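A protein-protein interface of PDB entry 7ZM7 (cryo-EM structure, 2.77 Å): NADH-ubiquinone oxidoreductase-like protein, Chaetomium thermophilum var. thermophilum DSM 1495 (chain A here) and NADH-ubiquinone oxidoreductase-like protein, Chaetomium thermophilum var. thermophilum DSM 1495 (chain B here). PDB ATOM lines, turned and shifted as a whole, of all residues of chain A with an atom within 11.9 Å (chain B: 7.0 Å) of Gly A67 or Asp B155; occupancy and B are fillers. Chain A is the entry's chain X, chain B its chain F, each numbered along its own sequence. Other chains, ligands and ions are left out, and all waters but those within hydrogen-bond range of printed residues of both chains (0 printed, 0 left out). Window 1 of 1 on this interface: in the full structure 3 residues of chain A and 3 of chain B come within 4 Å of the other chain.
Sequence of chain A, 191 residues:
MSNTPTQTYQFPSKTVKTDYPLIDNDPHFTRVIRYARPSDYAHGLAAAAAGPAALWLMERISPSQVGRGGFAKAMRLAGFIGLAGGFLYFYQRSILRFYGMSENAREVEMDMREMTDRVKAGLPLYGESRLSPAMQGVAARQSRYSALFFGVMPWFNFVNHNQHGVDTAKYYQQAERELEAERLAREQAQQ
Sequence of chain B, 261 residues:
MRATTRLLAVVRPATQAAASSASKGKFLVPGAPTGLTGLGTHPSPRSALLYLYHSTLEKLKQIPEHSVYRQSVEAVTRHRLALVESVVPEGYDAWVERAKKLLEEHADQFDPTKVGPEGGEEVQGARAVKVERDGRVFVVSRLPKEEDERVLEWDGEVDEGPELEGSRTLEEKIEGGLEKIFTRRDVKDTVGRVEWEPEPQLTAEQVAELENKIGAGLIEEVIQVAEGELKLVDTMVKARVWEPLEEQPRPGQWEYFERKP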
ATOM      1  N   GLU A  59       6.776   4.687 -15.329  1.00  0.00           N
ATOM      2  CA  GLU A  59       5.331   4.873 -15.619  1.00  0.00           C
ATOM      3  C   GLU A  59       5.025   4.454 -17.056  1.00  0.00           C
ATOM      4  O   GLU A  59       3.978   3.844 -17.285  1.00  0.00           O
ATOM      5  CB  GLU A  59       4.949   6.337 -15.413  1.00  0.00           C
ATOM      6  CG  GLU A  59       3.464   6.614 -15.546  1.00  0.00           C
ATOM      7  CD  GLU A  59       2.637   6.254 -14.326  1.00  0.00           C
ATOM      8  OE1 GLU A  59       1.412   6.478 -14.360  1.00  0.00           O
ATOM      9  OE2 GLU A  59       3.219   5.764 -13.342  1.00  0.00           O
ATOM     10  N   PRO A  63       2.879   1.013 -16.247  1.00  0.00           N
ATOM     11  CA  PRO A  63       1.988   2.052 -15.710  1.00  0.00           C
ATOM     12  C   PRO A  63       1.420   1.852 -14.295  1.00  0.00           C
ATOM     13  O   PRO A  63       1.074   0.742 -13.961  1.00  0.00           O
ATOM     14  CB  PRO A  63       0.927   2.178 -16.810  1.00  0.00           C
ATOM     15  CG  PRO A  63       1.590   1.644 -18.056  1.00  0.00           C
ATOM     16  CD  PRO A  63       2.461   0.517 -17.556  1.00  0.00           C
ATOM     17  N   SER A  64       1.332   2.928 -13.512  1.00  0.00           N
ATOM     18  CA  SER A  64       0.826   2.874 -12.113  1.00  0.00           C
ATOM     19  C   SER A  64      -0.681   2.680 -12.030  1.00  0.00           C
ATOM     20  O   SER A  64      -1.119   2.179 -10.987  1.00  0.00           O
ATOM     21  CB  SER A  64       1.214   4.109 -11.383  1.00  0.00           C
ATOM     22  OG  SER A  64       0.567   5.244 -11.934  1.00  0.00           O
ATOM     23  N   GLN A  65      -1.438   3.117 -13.041  1.00  0.00           N
ATOM     24  CA  GLN A  65      -2.919   2.946 -13.059  1.00  0.00           C
ATOM     25  C   GLN A  65      -3.527   3.885 -12.034  1.00  0.00           C
ATOM     26  O   GLN A  65      -4.651   3.626 -11.595  1.00  0.00           O
ATOM     27  CB  GLN A  65      -3.349   1.482 -12.898  1.00  0.00           C
ATOM     28  CG  GLN A  65      -2.693   0.539 -13.893  1.00  0.00           C
ATOM     29  CD  GLN A  65      -2.943   0.981 -15.311  1.00  0.00           C
ATOM     30  OE1 GLN A  65      -4.075   1.243 -15.708  1.00  0.00           O
ATOM     31  NE2 GLN A  65      -1.880   1.053 -16.093  1.00  0.00           N
ATOM     32  N   VAL A  66      -2.797   4.938 -11.685  1.00  0.00           N
ATOM     33  CA  VAL A  66      -3.247   5.906 -10.646  1.00  0.00           C
ATOM     34  C   VAL A  66      -4.289   6.840 -11.247  1.00  0.00           C
ATOM     35  O   VAL A  66      -4.455   6.808 -12.483  1.00  0.00           O
ATOM     36  CB  VAL A  66      -2.037   6.706 -10.139  1.00  0.00           C
ATOM     37  CG1 VAL A  66      -1.525   7.697 -11.168  1.00  0.00           C
ATOM     38  CG2 VAL A  66      -2.236   7.375  -8.795  1.00  0.00           C
ATOM     39  N   GLY A  67      -4.968   7.625 -10.414  1.00  0.00           N
ATOM     40  CA  GLY A  67      -5.949   8.609 -10.826  1.00  0.00           C
ATOM     41  C   GLY A  67      -5.368   9.815 -11.522  1.00  0.00           C
ATOM     42  O   GLY A  67      -4.214   9.792 -11.950  1.00  0.00           O
ATOM     43  N   ARG A  68      -6.152  10.888 -11.626  1.00  0.00           N
ATOM     44  CA  ARG A  68      -5.825  11.966 -12.552  1.00  0.00           C
ATOM     45  C   ARG A  68      -4.604  12.758 -12.111  1.00  0.00           C
ATOM     46  O   ARG A  68      -3.692  12.997 -12.910  1.00  0.00           O
ATOM     47  CB  ARG A  68      -7.017  12.897 -12.721  1.00  0.00           C
ATOM     48  CG  ARG A  68      -8.113  12.348 -13.595  1.00  0.00           C
ATOM     49  CD  ARG A  68      -9.138  13.425 -13.920  1.00  0.00           C
ATOM     50  NE  ARG A  68     -10.239  12.910 -14.727  1.00  0.00           N
ATOM     51  CZ  ARG A  68     -11.410  12.529 -14.232  1.00  0.00           C
ATOM     52  NH1 ARG A  68     -11.637  12.609 -12.929  1.00  0.00           N
ATOM     53  NH2 ARG A  68     -12.358  12.072 -15.038  1.00  0.00           N
ATOM     54  N   GLY A  69      -4.565  13.197 -10.866  1.00  0.00           N
ATOM     55  CA  GLY A  69      -3.464  14.051 -10.486  1.00  0.00           C
ATOM     56  C   GLY A  69      -2.299  13.383  -9.808  1.00  0.00           C
ATOM     57  O   GLY A  69      -1.359  14.073  -9.424  1.00  0.00           O
ATOM     58  N   GLY A  70      -2.326  12.062  -9.656  1.00  0.00           N
ATOM     59  CA  GLY A  70      -1.345  11.397  -8.821  1.00  0.00           C
ATOM     60  C   GLY A  70       0.065  11.445  -9.377  1.00  0.00           C
ATOM     61  O   GLY A  70       1.032  11.533  -8.622  1.00  0.00           O
ATOM     62  N   PHE A  71       0.212  11.359 -10.693  1.00  0.00           N
ATOM     63  CA  PHE A  71       1.562  11.329 -11.220  1.00  0.00           C
ATOM     64  C   PHE A  71       2.210  12.697 -11.155  1.00  0.00           C
ATOM     65  O   PHE A  71       3.418  12.794 -10.942  1.00  0.00           O
ATOM     66  CB  PHE A  71       1.591  10.797 -12.648  1.00  0.00           C
ATOM     67  CG  PHE A  71       2.949  10.352 -13.077  1.00  0.00           C
ATOM     68  CD1 PHE A  71       3.544   9.258 -12.479  1.00  0.00           C
ATOM     69  CD2 PHE A  71       3.659  11.048 -14.029  1.00  0.00           C
ATOM     70  CE1 PHE A  71       4.801   8.861 -12.842  1.00  0.00           C
ATOM     71  CE2 PHE A  71       4.912  10.644 -14.394  1.00  0.00           C
ATOM     72  CZ  PHE A  71       5.482   9.554 -13.803  1.00  0.00           C
ATOM     73  N   ALA A  72       1.432  13.762 -11.328  1.00  0.00           N
ATOM     74  CA  ALA A  72       1.976  15.105 -11.180  1.00  0.00           C
ATOM     75  C   ALA A  72       2.492  15.342  -9.768  1.00  0.00           C
ATOM     76  O   ALA A  72       3.530  15.977  -9.577  1.00  0.00           O
ATOM     77  CB  ALA A  72       0.911  16.131 -11.540  1.00  0.00           C
ATOM     78  N   LYS A  73       1.777  14.837  -8.767  1.00  0.00           N
ATOM     79  CA  LYS A  73       2.253  14.931  -7.397  1.00  0.00           C
ATOM     80  C   LYS A  73       3.572  14.187  -7.212  1.00  0.00           C
ATOM     81  O   LYS A  73       4.513  14.718  -6.610  1.00  0.00           O
ATOM     82  CB  LYS A  73       1.185  14.388  -6.458  1.00  0.00           C
ATOM     83  CG  LYS A  73       1.520  14.495  -5.003  1.00  0.00           C
ATOM     84  CD  LYS A  73       0.504  13.759  -4.170  1.00  0.00           C
ATOM     85  CE  LYS A  73       0.836  13.808  -2.699  1.00  0.00           C
ATOM     86  NZ  LYS A  73       1.347  15.134  -2.278  1.00  0.00           N
ATOM     87  N   ALA A  74       3.658  12.964  -7.744  1.00  0.00           N
ATOM     88  CA  ALA A  74       4.862  12.152  -7.620  1.00  0.00           C
ATOM     89  C   ALA A  74       6.040  12.765  -8.369  1.00  0.00           C
ATOM     90  O   ALA A  74       7.165  12.755  -7.870  1.00  0.00           O
ATOM     91  CB  ALA A  74       4.580  10.734  -8.116  1.00  0.00           C
ATOM     92  N   MET A  75       5.799  13.288  -9.573  1.00  0.00           N
ATOM     93  CA  MET A  75       6.838  13.989 -10.320  1.00  0.00           C
ATOM     94  C   MET A  75       7.455  15.132  -9.531  1.00  0.00           C
ATOM     95  O   MET A  75       8.656  15.390  -9.652  1.00  0.00           O
ATOM     96  CB  MET A  75       6.273  14.509 -11.634  1.00  0.00           C
ATOM     97  CG  MET A  75       5.962  13.475 -12.662  1.00  0.00           C
ATOM     98  SD  MET A  75       7.424  13.136 -13.664  1.00  0.00           S
ATOM     99  CE  MET A  75       8.008  11.611 -12.965  1.00  0.00           C
ATOM    100  N   ARG A  76       6.645  15.846  -8.763  1.00  0.00           N
ATOM    101  CA  ARG A  76       7.169  16.942  -7.905  1.00  0.00           C
ATOM    102  C   ARG A  76       8.110  16.370  -6.841  1.00  0.00           C
ATOM    103  O   ARG A  76       9.137  17.007  -6.584  1.00  0.00           O
ATOM    104  CB  ARG A  76       6.047  17.874  -7.444  1.00  0.00           C
ATOM    105  CG  ARG A  76       5.453  18.694  -8.578  1.00  0.00           C
ATOM    106  CD  ARG A  76       4.418  19.696  -8.116  1.00  0.00           C
ATOM    107  NE  ARG A  76       3.233  19.079  -7.546  1.00  0.00           N
ATOM    108  CZ  ARG A  76       2.124  18.811  -8.220  1.00  0.00           C
ATOM    109  NH1 ARG A  76       2.045  19.101  -9.506  1.00  0.00           N
ATOM    110  NH2 ARG A  76       1.095  18.260  -7.605  1.00  0.00           N
ATOM    111  N   VAL B 123     -19.604   3.024 -13.292  1.00  0.00           N
ATOM    112  CA  VAL B 123     -20.138   4.296 -12.822  1.00  0.00           C
ATOM    113  C   VAL B 123     -19.165   5.447 -13.009  1.00  0.00           C
ATOM    114  O   VAL B 123     -19.584   6.606 -12.956  1.00  0.00           O
ATOM    115  CB  VAL B 123     -20.542   4.195 -11.340  1.00  0.00           C
ATOM    116  CG1 VAL B 123     -21.631   3.159 -11.165  1.00  0.00           C
ATOM    117  CG2 VAL B 123     -19.339   3.858 -10.489  1.00  0.00           C
ATOM    118  N   GLN B 124     -17.882   5.169 -13.221  1.00  0.00           N
ATOM    119  CA  GLN B 124     -16.934   6.232 -13.522  1.00  0.00           C
ATOM    120  C   GLN B 124     -16.972   6.643 -14.985  1.00  0.00           C
ATOM    121  O   GLN B 124     -16.304   7.611 -15.358  1.00  0.00           O
ATOM    122  CB  GLN B 124     -15.504   5.824 -13.147  1.00  0.00           C
ATOM    123  CG  GLN B 124     -14.904   4.716 -13.995  1.00  0.00           C
ATOM    124  CD  GLN B 124     -14.790   3.402 -13.251  1.00  0.00           C
ATOM    125  OE1 GLN B 124     -15.543   3.136 -12.316  1.00  0.00           O
ATOM    126  NE2 GLN B 124     -13.837   2.573 -13.659  1.00  0.00           N
ATOM    127  N   GLY B 125     -17.735   5.934 -15.819  1.00  0.00           N
ATOM    128  CA  GLY B 125     -17.900   6.287 -17.208  1.00  0.00           C
ATOM    129  C   GLY B 125     -19.324   6.739 -17.487  1.00  0.00           C
ATOM    130  O   GLY B 125     -20.252   6.467 -16.716  1.00  0.00           O
ATOM    131  N   PRO B 144     -21.155  10.607 -14.369  1.00  0.00           N
ATOM    132  CA  PRO B 144     -20.311  10.399 -13.189  1.00  0.00           C
ATOM    133  C   PRO B 144     -20.175  11.679 -12.380  1.00  0.00           C
ATOM    134  O   PRO B 144     -20.025  12.770 -12.933  1.00  0.00           O
ATOM    135  CB  PRO B 144     -18.970   9.960 -13.784  1.00  0.00           C
ATOM    136  CG  PRO B 144     -19.323   9.380 -15.105  1.00  0.00           C
ATOM    137  CD  PRO B 144     -20.491  10.171 -15.608  1.00  0.00           C
ATOM    138  N   GLU B 149     -10.242  16.225  -7.434  1.00  0.00           N
ATOM    139  CA  GLU B 149      -9.135  15.342  -7.753  1.00  0.00           C
ATOM    140  C   GLU B 149      -8.312  14.987  -6.527  1.00  0.00           C
ATOM    141  O   GLU B 149      -7.710  13.911  -6.498  1.00  0.00           O
ATOM    142  CB  GLU B 149      -8.238  15.995  -8.800  1.00  0.00           C
ATOM    143  CG  GLU B 149      -8.898  16.157 -10.153  1.00  0.00           C
ATOM    144  CD  GLU B 149      -9.770  17.393 -10.222  1.00  0.00           C
ATOM    145  OE1 GLU B 149      -9.804  18.151  -9.229  1.00  0.00           O
ATOM    146  OE2 GLU B 149     -10.426  17.603 -11.264  1.00  0.00           O
ATOM    147  N   LEU B 152     -10.166  11.825  -4.969  1.00  0.00           N
ATOM    148  CA  LEU B 152     -10.675  10.749  -5.807  1.00  0.00           C
ATOM    149  C   LEU B 152      -9.600   9.683  -6.006  1.00  0.00           C
ATOM    150  O   LEU B 152      -8.543   9.965  -6.574  1.00  0.00           O
ATOM    151  CB  LEU B 152     -11.133  11.333  -7.140  1.00  0.00           C
ATOM    152  CG  LEU B 152     -12.112  10.545  -7.985  1.00  0.00           C
ATOM    153  CD1 LEU B 152     -13.380  10.393  -7.206  1.00  0.00           C
ATOM    154  CD2 LEU B 152     -12.384  11.304  -9.240  1.00  0.00           C
ATOM    155  N   GLU B 153      -9.872   8.460  -5.548  1.00  0.00           N
ATOM    156  CA  GLU B 153      -8.965   7.328  -5.704  1.00  0.00           C
ATOM    157  C   GLU B 153      -9.315   6.536  -6.953  1.00  0.00           C
ATOM    158  O   GLU B 153     -10.456   6.088  -7.105  1.00  0.00           O
ATOM    159  CB  GLU B 153      -9.029   6.387  -4.507  1.00  0.00           C
ATOM    160  CG  GLU B 153      -8.317   6.844  -3.261  1.00  0.00           C
ATOM    161  CD  GLU B 153      -8.884   6.185  -2.031  1.00  0.00           C
ATOM    162  OE1 GLU B 153      -9.993   5.634  -2.135  1.00  0.00           O
ATOM    163  OE2 GLU B 153      -8.234   6.205  -0.972  1.00  0.00           O
ATOM    164  N   TRP B 154      -8.325   6.332  -7.820  1.00  0.00           N
ATOM    165  CA  TRP B 154      -8.469   5.506  -9.020  1.00  0.00           C
ATOM    166  C   TRP B 154      -9.563   6.031  -9.939  1.00  0.00           C
ATOM    167  O   TRP B 154     -10.305   5.264 -10.545  1.00  0.00           O
ATOM    168  CB  TRP B 154      -8.735   4.044  -8.668  1.00  0.00           C
ATOM    169  CG  TRP B 154      -7.574   3.328  -8.092  1.00  0.00           C
ATOM    170  CD1 TRP B 154      -6.443   2.967  -8.738  1.00  0.00           C
ATOM    171  CD2 TRP B 154      -7.438   2.865  -6.752  1.00  0.00           C
ATOM    172  NE1 TRP B 154      -5.604   2.314  -7.885  1.00  0.00           N
ATOM    173  CE2 TRP B 154      -6.193   2.237  -6.655  1.00  0.00           C
ATOM    174  CE3 TRP B 154      -8.246   2.937  -5.615  1.00  0.00           C
ATOM    175  CZ2 TRP B 154      -5.736   1.677  -5.477  1.00  0.00           C
ATOM    176  CZ3 TRP B 154      -7.787   2.395  -4.445  1.00  0.00           C
ATOM    177  CH2 TRP B 154      -6.546   1.767  -4.385  1.00  0.00           C
ATOM    178  N   ASP B 155      -9.667   7.353 -10.030  1.00  0.00           N
ATOM    179  CA  ASP B 155     -10.665   8.014 -10.864  1.00  0.00           C
ATOM    180  C   ASP B 155     -12.077   7.632 -10.457  1.00  0.00           C
ATOM    181  O   ASP B 155     -13.010   7.724 -11.251  1.00  0.00           O
ATOM    182  CB  ASP B 155     -10.439   7.717 -12.349  1.00  0.00           C
ATOM    183  CG  ASP B 155      -9.358   8.580 -12.955  1.00  0.00           C
ATOM    184  OD1 ASP B 155      -8.892   9.512 -12.274  1.00  0.00           O
ATOM    185  OD2 ASP B 155      -8.977   8.331 -14.116  1.00  0.00           O
ATOM    186  N   GLY B 156     -12.246   7.205  -9.219  1.00  0.00           N
ATOM    187  CA  GLY B 156     -13.550   6.841  -8.728  1.00  0.00           C
ATOM    188  C   GLY B 156     -13.994   5.427  -9.001  1.00  0.00           C
ATOM    189  O   GLY B 156     -15.149   5.106  -8.721  1.00  0.00           O
ATOM    190  N   GLU B 157     -13.129   4.567  -9.522  1.00  0.00           N
ATOM    191  CA  GLU B 157     -13.529   3.190  -9.760  1.00  0.00           C
ATOM    192  C   GLU B 157     -13.919   2.524  -8.455  1.00  0.00           C
ATOM    193  O   GLU B 157     -13.145   2.519  -7.496  1.00  0.00           O
ATOM    194  CB  GLU B 157     -12.413   2.391 -10.426  1.00  0.00           C
ATOM    195  CG  GLU B 157     -12.816   0.934 -10.594  1.00  0.00           C
ATOM    196  CD  GLU B 157     -11.957   0.146 -11.544  1.00  0.00           C
ATOM    197  OE1 GLU B 157     -11.059   0.721 -12.174  1.00  0.00           O
ATOM    198  OE2 GLU B 157     -12.189  -1.066 -11.652  1.00  0.00           O
ATOM    199  N   VAL B 158     -15.122   1.948  -8.429  1.00  0.00           N
ATOM    200  CA  VAL B 158     -15.634   1.354  -7.204  1.00  0.00           C
ATOM    201  C   VAL B 158     -14.705   0.243  -6.748  1.00  0.00           C
ATOM    202  O   VAL B 158     -14.180  -0.534  -7.556  1.00  0.00           O
ATOM    203  CB  VAL B 158     -17.068   0.842  -7.412  1.00  0.00           C
ATOM    204  CG1 VAL B 158     -17.124  -0.175  -8.544  1.00  0.00           C
ATOM    205  CG2 VAL B 158     -17.611   0.244  -6.124  1.00  0.00           C
ATOM    206  N   VAL B 187     -12.178   2.316 -18.542  1.00  0.00           N
ATOM    207  CA  VAL B 187     -12.939   3.549 -18.718  1.00  0.00           C
ATOM    208  C   VAL B 187     -12.357   4.375 -19.852  1.00  0.00           C
ATOM    209  O   VAL B 187     -13.077   5.121 -20.525  1.00  0.00           O
ATOM    210  CB  VAL B 187     -12.987   4.340 -17.399  1.00  0.00           C
ATOM    211  CG1 VAL B 187     -11.598   4.803 -17.002  1.00  0.00           C
ATOM    212  CG2 VAL B 187     -13.936   5.518 -17.518  1.00  0.00           C
ATOM    213  N   LYS B 188     -11.053   4.248 -20.093  1.00  0.00           N
ATOM    214  CA  LYS B 188     -10.414   4.935 -21.200  1.00  0.00           C
ATOM    215  C   LYS B 188     -10.669   4.255 -22.532  1.00  0.00           C
ATOM    216  O   LYS B 188     -10.458   4.877 -23.575  1.00  0.00           O
ATOM    217  CB  LYS B 188      -8.914   5.040 -20.926  1.00  0.00           C
ATOM    218  CG  LYS B 188      -8.586   5.950 -19.745  1.00  0.00           C
ATOM    219  CD  LYS B 188      -7.091   6.179 -19.581  1.00  0.00           C
ATOM    220  CE  LYS B 188      -6.397   4.951 -19.020  1.00  0.00           C
ATOM    221  NZ  LYS B 188      -4.953   5.203 -18.751  1.00  0.00           N
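N of Arg A68 is in hydrogen-bond range of OD1 of Asp B155 (3.1 Å).
Among the printed residues, merely in contact across the chains: Gln A65 with Trp B154, Gly A67 with Asp B155 and Arg A68 with Leu B152.
Of chain A, only Gly A67 (3.4 Å) and Arg A68 (3.1 Å) come within 4 Å of Asp B155. Gln B124 touches none of the printed residues of chain A. Of the printed residues of chain A, Trp B154 touches Gln A65 (3.4 Å). Printed residues of chain B within 4 Å of Arg A68: Leu B152 and Asp B155. Of the printed residues of chain A, Leu B152 touches Arg A68. Of the printed residues of chain B, Gln A65 touches Trp B154 (3.4 Å). Lys B188 touches none of the printed residues of chain A. The nearest residue of chain B that does not touch Gly A67 is Trp B154 (4.3 Å). The nearest printed residue of chain B that does not touch Gln A65 is Lys B188 (5.1 Å).
Printed residues of chain B that touch a printed residue of chain A: Leu B152, Trp B154 and Asp B155. Along chain B the printed residues that touch a printed residue of chain A span positions 152 to 155. Among the printed residues, 4 pairs touch across the chains.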
